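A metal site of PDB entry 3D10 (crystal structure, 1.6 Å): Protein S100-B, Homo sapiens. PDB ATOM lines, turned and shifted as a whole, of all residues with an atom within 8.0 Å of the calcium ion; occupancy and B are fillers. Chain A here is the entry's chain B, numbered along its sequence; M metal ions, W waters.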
ATOM      1  N   PHE A  15     -22.750 -21.141  12.987  1.00  0.00           N
ATOM      2  CA  PHE A  15     -21.372 -20.967  13.528  1.00  0.00           C
ATOM      3  C   PHE A  15     -20.919 -22.148  14.409  1.00  0.00           C
ATOM      4  O   PHE A  15     -19.786 -22.622  14.279  1.00  0.00           O
ATOM      5  CB  PHE A  15     -21.291 -19.673  14.340  1.00  0.00           C
ATOM      6  CG  PHE A  15     -19.905 -19.451  14.987  1.00  0.00           C
ATOM      7  CD1 PHE A  15     -18.866 -18.900  14.219  1.00  0.00           C
ATOM      8  CD2 PHE A  15     -19.656 -19.790  16.307  1.00  0.00           C
ATOM      9  CE1 PHE A  15     -17.580 -18.694  14.746  1.00  0.00           C
ATOM     10  CE2 PHE A  15     -18.404 -19.567  16.853  1.00  0.00           C
ATOM     11  CZ  PHE A  15     -17.359 -19.032  16.067  1.00  0.00           C
ATOM     12  N   HIS A  16     -21.730 -22.571  15.359  1.00  0.00           N
ATOM     13  CA  HIS A  16     -21.335 -23.622  16.285  1.00  0.00           C
ATOM     14  C   HIS A  16     -21.262 -24.972  15.571  1.00  0.00           C
ATOM     15  O   HIS A  16     -20.492 -25.877  15.954  1.00  0.00           O
ATOM     16  CB  HIS A  16     -22.327 -23.691  17.462  1.00  0.00           C
ATOM     17  CG  HIS A  16     -22.206 -22.562  18.432  1.00  0.00           C
ATOM     18  ND1 HIS A  16     -22.543 -21.262  18.091  1.00  0.00           N
ATOM     19  CD2 HIS A  16     -21.709 -22.502  19.674  1.00  0.00           C
ATOM     20  CE1 HIS A  16     -22.336 -20.479  19.133  1.00  0.00           C
ATOM     21  NE2 HIS A  16     -21.822 -21.208  20.097  1.00  0.00           N
ATOM     22  N   GLN A  17     -22.095 -25.108  14.543  1.00  0.00           N
ATOM     23  CA  GLN A  17     -22.115 -26.345  13.772  1.00  0.00           C
ATOM     24  C   GLN A  17     -20.702 -26.581  13.238  1.00  0.00           C
ATOM     25  O   GLN A  17     -20.179 -27.711  13.283  1.00  0.00           O
ATOM     26  CB  GLN A  17     -23.119 -26.220  12.609  1.00  0.00           C
ATOM     27  CG  GLN A  17     -24.561 -26.684  12.893  1.00  0.00           C
ATOM     28  CD  GLN A  17     -25.585 -26.200  11.812  1.00  0.00           C
ATOM     29  OE1 GLN A  17     -25.279 -26.028  10.602  1.00  0.00           O
ATOM     30  NE2 GLN A  17     -26.820 -26.004  12.266  1.00  0.00           N
ATOM     31  N   TYR A  18     -20.092 -25.497  12.739  1.00  0.00           N
ATOM     32  CA  TYR A  18     -18.804 -25.589  12.076  1.00  0.00           C
ATOM     33  C   TYR A  18     -17.648 -25.427  13.034  1.00  0.00           C
ATOM     34  O   TYR A  18     -16.617 -26.168  12.973  1.00  0.00           O
ATOM     35  CB  TYR A  18     -18.728 -24.619  10.888  1.00  0.00           C
ATOM     36  CG  TYR A  18     -19.454 -25.150   9.726  1.00  0.00           C
ATOM     37  CD1 TYR A  18     -20.817 -24.985   9.613  1.00  0.00           C
ATOM     38  CD2 TYR A  18     -18.777 -25.945   8.786  1.00  0.00           C
ATOM     39  CE1 TYR A  18     -21.512 -25.548   8.490  1.00  0.00           C
ATOM     40  CE2 TYR A  18     -19.463 -26.538   7.716  1.00  0.00           C
ATOM     41  CZ  TYR A  18     -20.811 -26.339   7.594  1.00  0.00           C
ATOM     42  OH  TYR A  18     -21.418 -26.881   6.519  1.00  0.00           O
ATOM     43  N   SER A  19     -17.819 -24.548  13.982  1.00  0.00           N
ATOM     44  CA  SER A  19     -16.682 -24.298  14.934  1.00  0.00           C
ATOM     45  C   SER A  19     -16.370 -25.516  15.850  1.00  0.00           C
ATOM     46  O   SER A  19     -15.210 -25.742  16.273  1.00  0.00           O
ATOM     47  CB  SER A  19     -16.897 -22.999  15.774  1.00  0.00           C
ATOM     48  OG  SER A  19     -17.986 -23.131  16.683  1.00  0.00           O
ATOM     49  N   GLY A  20     -17.401 -26.295  16.159  1.00  0.00           N
ATOM     50  CA  GLY A  20     -17.246 -27.480  17.053  1.00  0.00           C
ATOM     51  C   GLY A  20     -16.782 -28.749  16.332  1.00  0.00           C
ATOM     52  O   GLY A  20     -16.872 -29.841  16.876  1.00  0.00           O
ATOM     53  N   ARG A  21     -16.324 -28.625  15.073  1.00  0.00           N
ATOM     54  CA  ARG A  21     -15.807 -29.823  14.378  1.00  0.00           C
ATOM     55  C   ARG A  21     -14.461 -30.310  14.934  1.00  0.00           C
ATOM     56  O   ARG A  21     -14.247 -31.530  15.185  1.00  0.00           O
ATOM     57  CB  ARG A  21     -15.744 -29.563  12.871  1.00  0.00           C
ATOM     58  CG  ARG A  21     -17.145 -29.473  12.286  1.00  0.00           C
ATOM     59  CD  ARG A  21     -17.070 -29.331  10.806  1.00  0.00           C
ATOM     60  NE  ARG A  21     -18.343 -29.502  10.131  1.00  0.00           N
ATOM     61  CZ  ARG A  21     -18.448 -29.568   8.813  1.00  0.00           C
ATOM     62  NH1 ARG A  21     -19.616 -29.736   8.231  1.00  0.00           N
ATOM     63  NH2 ARG A  21     -17.357 -29.518   8.087  1.00  0.00           N
ATOM     64  N   GLU A  22     -13.588 -29.358  15.200  1.00  0.00           N
ATOM     65  CA  GLU A  22     -12.197 -29.641  15.470  1.00  0.00           C
ATOM     66  C   GLU A  22     -11.587 -28.526  16.334  1.00  0.00           C
ATOM     67  O   GLU A  22     -12.065 -27.399  16.329  1.00  0.00           O
ATOM     68  CB  GLU A  22     -11.418 -29.745  14.146  1.00  0.00           C
ATOM     69  CG  GLU A  22     -11.820 -30.936  13.251  1.00  0.00           C
ATOM     70  CD  GLU A  22     -10.798 -31.203  12.130  1.00  0.00           C
ATOM     71  OE1 GLU A  22     -11.193 -31.235  10.916  1.00  0.00           O
ATOM     72  OE2 GLU A  22      -9.597 -31.357  12.483  1.00  0.00           O
ATOM     73  N   GLY A  23     -10.544 -28.869  17.083  1.00  0.00           N
ATOM     74  CA  GLY A  23      -9.761 -27.877  17.813  1.00  0.00           C
ATOM     75  C   GLY A  23     -10.649 -27.154  18.809  1.00  0.00           C
ATOM     76  O   GLY A  23     -11.575 -27.750  19.370  1.00  0.00           O
ATOM     77  N   ASP A  24     -10.394 -25.866  19.006  1.00  0.00           N
ATOM     78  CA  ASP A  24     -11.277 -25.055  19.822  1.00  0.00           C
ATOM     79  C   ASP A  24     -12.696 -25.280  19.337  1.00  0.00           C
ATOM     80  O   ASP A  24     -12.940 -25.108  18.166  1.00  0.00           O
ATOM     81  CB  ASP A  24     -10.867 -23.597  19.690  1.00  0.00           C
ATOM     82  CG  ASP A  24     -11.588 -22.685  20.669  1.00  0.00           C
ATOM     83  OD1 ASP A  24     -12.765 -22.885  20.982  1.00  0.00           O
ATOM     84  OD2 ASP A  24     -10.965 -21.727  21.124  1.00  0.00           O
ATOM     85  N   LYS A  25     -13.624 -25.679  20.205  1.00  0.00           N
ATOM     86  CA  LYS A  25     -15.026 -25.872  19.755  1.00  0.00           C
ATOM     87  C   LYS A  25     -15.801 -24.570  19.565  1.00  0.00           C
ATOM     88  O   LYS A  25     -16.967 -24.566  19.161  1.00  0.00           O
ATOM     89  CB  LYS A  25     -15.737 -26.812  20.727  1.00  0.00           C
ATOM     90  CG  LYS A  25     -15.219 -28.242  20.607  1.00  0.00           C
ATOM     91  CD  LYS A  25     -15.864 -29.160  21.607  1.00  0.00           C
ATOM     92  CE  LYS A  25     -16.085 -30.528  20.977  1.00  0.00           C
ATOM     93  NZ  LYS A  25     -14.835 -31.185  20.528  1.00  0.00           N
ATOM     94  N   HIS A  26     -15.152 -23.449  19.782  1.00  0.00           N
ATOM     95  CA  HIS A  26     -15.838 -22.175  19.782  1.00  0.00           C
ATOM     96  C   HIS A  26     -15.197 -21.202  18.816  1.00  0.00           C
ATOM     97  O   HIS A  26     -15.495 -20.004  18.819  1.00  0.00           O
ATOM     98  CB  HIS A  26     -15.890 -21.635  21.214  1.00  0.00           C
ATOM     99  CG  HIS A  26     -17.110 -20.834  21.513  1.00  0.00           C
ATOM    100  ND1 HIS A  26     -17.202 -20.005  22.611  1.00  0.00           N
ATOM    101  CD2 HIS A  26     -18.288 -20.729  20.859  1.00  0.00           C
ATOM    102  CE1 HIS A  26     -18.390 -19.423  22.614  1.00  0.00           C
ATOM    103  NE2 HIS A  26     -19.063 -19.843  21.549  1.00  0.00           N
ATOM    104  N   LYS A  27     -14.345 -21.732  17.932  1.00  0.00           N
ATOM    105  CA  LYS A  27     -13.762 -20.904  16.898  1.00  0.00           C
ATOM    106  C   LYS A  27     -13.623 -21.732  15.638  1.00  0.00           C
ATOM    107  O   LYS A  27     -13.438 -22.918  15.752  1.00  0.00           O
ATOM    108  CB  LYS A  27     -12.407 -20.339  17.341  1.00  0.00           C
ATOM    109  CG  LYS A  27     -12.465 -19.550  18.668  1.00  0.00           C
ATOM    110  CD  LYS A  27     -11.152 -19.038  19.134  1.00  0.00           C
ATOM    111  CE  LYS A  27     -11.382 -18.262  20.443  1.00  0.00           C
ATOM    112  NZ  LYS A  27     -11.764 -19.113  21.640  1.00  0.00           N
ATOM    113  N   LEU A  28     -13.749 -21.109  14.449  1.00  0.00           N
ATOM    114  CA  LEU A  28     -13.508 -21.799  13.174  1.00  0.00           C
ATOM    115  C   LEU A  28     -12.035 -21.800  12.808  1.00  0.00           C
ATOM    116  O   LEU A  28     -11.424 -20.710  12.787  1.00  0.00           O
ATOM    117  CB  LEU A  28     -14.275 -21.141  12.042  1.00  0.00           C
ATOM    118  CG  LEU A  28     -15.755 -20.976  12.324  1.00  0.00           C
ATOM    119  CD1 LEU A  28     -16.344 -19.867  11.334  1.00  0.00           C
ATOM    120  CD2 LEU A  28     -16.463 -22.311  12.056  1.00  0.00           C
ATOM    121  N   LYS A  29     -11.461 -22.969  12.564  1.00  0.00           N
ATOM    122  CA  LYS A  29     -10.122 -22.973  11.977  1.00  0.00           C
ATOM    123  C   LYS A  29     -10.300 -22.935  10.467  1.00  0.00           C
ATOM    124  O   LYS A  29     -11.452 -22.977   9.968  1.00  0.00           O
ATOM    125  CB  LYS A  29      -9.269 -24.152  12.460  1.00  0.00           C
ATOM    126  CG  LYS A  29      -9.900 -25.546  12.424  1.00  0.00           C
ATOM    127  CD  LYS A  29      -8.969 -26.597  12.956  1.00  0.00           C
ATOM    128  CE  LYS A  29      -7.885 -26.050  13.955  1.00  0.00           C
ATOM    129  NZ  LYS A  29      -8.222 -25.625  15.408  1.00  0.00           N
ATOM    130  N   LYS A  30      -9.188 -22.858   9.730  1.00  0.00           N
ATOM    131  CA  LYS A  30      -9.280 -22.689   8.280  1.00  0.00           C
ATOM    132  C   LYS A  30     -10.173 -23.771   7.637  1.00  0.00           C
ATOM    133  O   LYS A  30     -11.038 -23.447   6.797  1.00  0.00           O
ATOM    134  CB  LYS A  30      -7.896 -22.674   7.622  1.00  0.00           C
ATOM    135  CG  LYS A  30      -7.125 -21.464   7.944  1.00  0.00           C
ATOM    136  CD  LYS A  30      -5.664 -21.633   7.468  1.00  0.00           C
ATOM    137  CE  LYS A  30      -4.783 -20.550   8.014  1.00  0.00           C
ATOM    138  NZ  LYS A  30      -3.830 -20.131   6.959  1.00  0.00           N
ATOM    139  N   SER A  31      -9.985 -25.017   8.052  1.00  0.00           N
ATOM    140  CA  SER A  31     -10.767 -26.078   7.380  1.00  0.00           C
ATOM    141  C   SER A  31     -12.247 -25.947   7.669  1.00  0.00           C
ATOM    142  O   SER A  31     -13.093 -26.122   6.798  1.00  0.00           O
ATOM    143  CB  SER A  31     -10.234 -27.491   7.709  1.00  0.00           C
ATOM    144  OG  SER A  31     -10.292 -27.793   9.091  1.00  0.00           O
ATOM    145  N   GLU A  32     -12.564 -25.559   8.890  1.00  0.00           N
ATOM    146  CA  GLU A  32     -13.973 -25.344   9.286  1.00  0.00           C
ATOM    147  C   GLU A  32     -14.577 -24.139   8.573  1.00  0.00           C
ATOM    148  O   GLU A  32     -15.678 -24.184   8.092  1.00  0.00           O
ATOM    149  CB  GLU A  32     -14.078 -25.154  10.816  1.00  0.00           C
ATOM    150  CG  GLU A  32     -13.660 -26.356  11.604  1.00  0.00           C
ATOM    151  CD  GLU A  32     -13.610 -26.153  13.120  1.00  0.00           C
ATOM    152  OE1 GLU A  32     -13.314 -25.041  13.599  1.00  0.00           O
ATOM    153  OE2 GLU A  32     -13.876 -27.121  13.854  1.00  0.00           O
ATOM    154  N   LEU A  33     -13.855 -23.038   8.508  1.00  0.00           N
ATOM    155  CA  LEU A  33     -14.233 -21.889   7.697  1.00  0.00           C
ATOM    156  C   LEU A  33     -14.463 -22.255   6.210  1.00  0.00           C
ATOM    157  O   LEU A  33     -15.460 -21.822   5.593  1.00  0.00           O
ATOM    158  CB  LEU A  33     -13.121 -20.803   7.865  1.00  0.00           C
ATOM    159  CG  LEU A  33     -13.364 -19.451   7.194  1.00  0.00           C
ATOM    160  CD1 LEU A  33     -14.763 -18.767   7.521  1.00  0.00           C
ATOM    161  CD2 LEU A  33     -12.217 -18.519   7.418  1.00  0.00           C
ATOM    162  N   GLU A  68      -7.557 -18.005  14.100  1.00  0.00           N
ATOM    163  CA  GLU A  68      -8.913 -18.558  13.987  1.00  0.00           C
ATOM    164  C   GLU A  68     -10.020 -17.496  13.923  1.00  0.00           C
ATOM    165  O   GLU A  68      -9.808 -16.328  14.159  1.00  0.00           O
ATOM    166  CB  GLU A  68      -9.164 -19.580  15.098  1.00  0.00           C
ATOM    167  CG  GLU A  68      -8.104 -20.713  15.115  1.00  0.00           C
ATOM    168  CD  GLU A  68      -8.623 -22.013  15.705  1.00  0.00           C
ATOM    169  OE1 GLU A  68      -9.848 -22.117  15.994  1.00  0.00           O
ATOM    170  OE2 GLU A  68      -7.799 -22.956  15.832  1.00  0.00           O
ATOM    171  N   CYS A  69     -11.219 -17.936  13.643  1.00  0.00           N
ATOM    172  CA  CYS A  69     -12.333 -16.988  13.521  1.00  0.00           C
ATOM    173  C   CYS A  69     -13.297 -17.258  14.681  1.00  0.00           C
ATOM    174  O   CYS A  69     -13.928 -18.352  14.734  1.00  0.00           O
ATOM    175  CB  CYS A  69     -13.090 -17.154  12.142  1.00  0.00           C
ATOM    176  SG  CYS A  69     -14.514 -16.009  11.954  1.00  0.00           S
HETATM  177 CA    CA M   1     -12.982 -25.371  15.793  1.00  0.00          CA
HETATM  178  O   HOH W   1     -10.770 -24.476  15.721  1.00  0.00           O
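Five residues have an atom within 4 Å of the calcium ion: Ser 19, Glu 22, Asp 24, Lys 27 and Glu 32.
The nearest printed residue that does not touch the calcium ion is Gly 23 (4.2 Å).
Water W1 lies within hydrogen-bond range of the side-chain carboxylate (OE1) of Glu 68 (2.5 Å) and the side-chain amino group (NZ) of Lys 29 (2.8 Å).
The side-chain carboxylate (OE1) of Glu 32 lies close to the backbone NH (N) of Lys 29 (3.0 Å).
The side-chain carboxylate (OE2) of Glu 32 lies close to the backbone NH (N) of Arg 21 (3.1 Å).
The backbone carbonyl oxygen (O) of Lys 25 lies within hydrogen-bond range of the side-chain hydroxyl (OG) of Ser 19 (3.0 Å).
The backbone carbonyl oxygen (O) of Phe 15 is in hydrogen-bond range of the side-chain hydroxyl (OG) of Ser 19, at 3.0 Å.
The side-chain carboxylate of Asp 24 lies within salt-bridge range of the side-chain amino group of Lys 27, at 2.8 Å.
The backbone NH (N) of His 26 lies within hydrogen-bond range of the side-chain carboxylate (OD1) of Asp 24 (2.7 Å).
The calcium ion is bound by the side-chain carboxylate (OE1) of Glu 32 (2.2 Å), the backbone carbonyl oxygen (O) of Glu 22 (2.3 Å), the backbone carbonyl oxygen (O) of Ser 19 (2.3 Å), water W1 (2.4 Å), the backbone carbonyl oxygen (O) of Asp 24 (2.4 Å), the backbone carbonyl oxygen (O) of Lys 27 (2.5 Å) and the side-chain carboxylate (OE2) of Glu 32 (2.8 Å).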
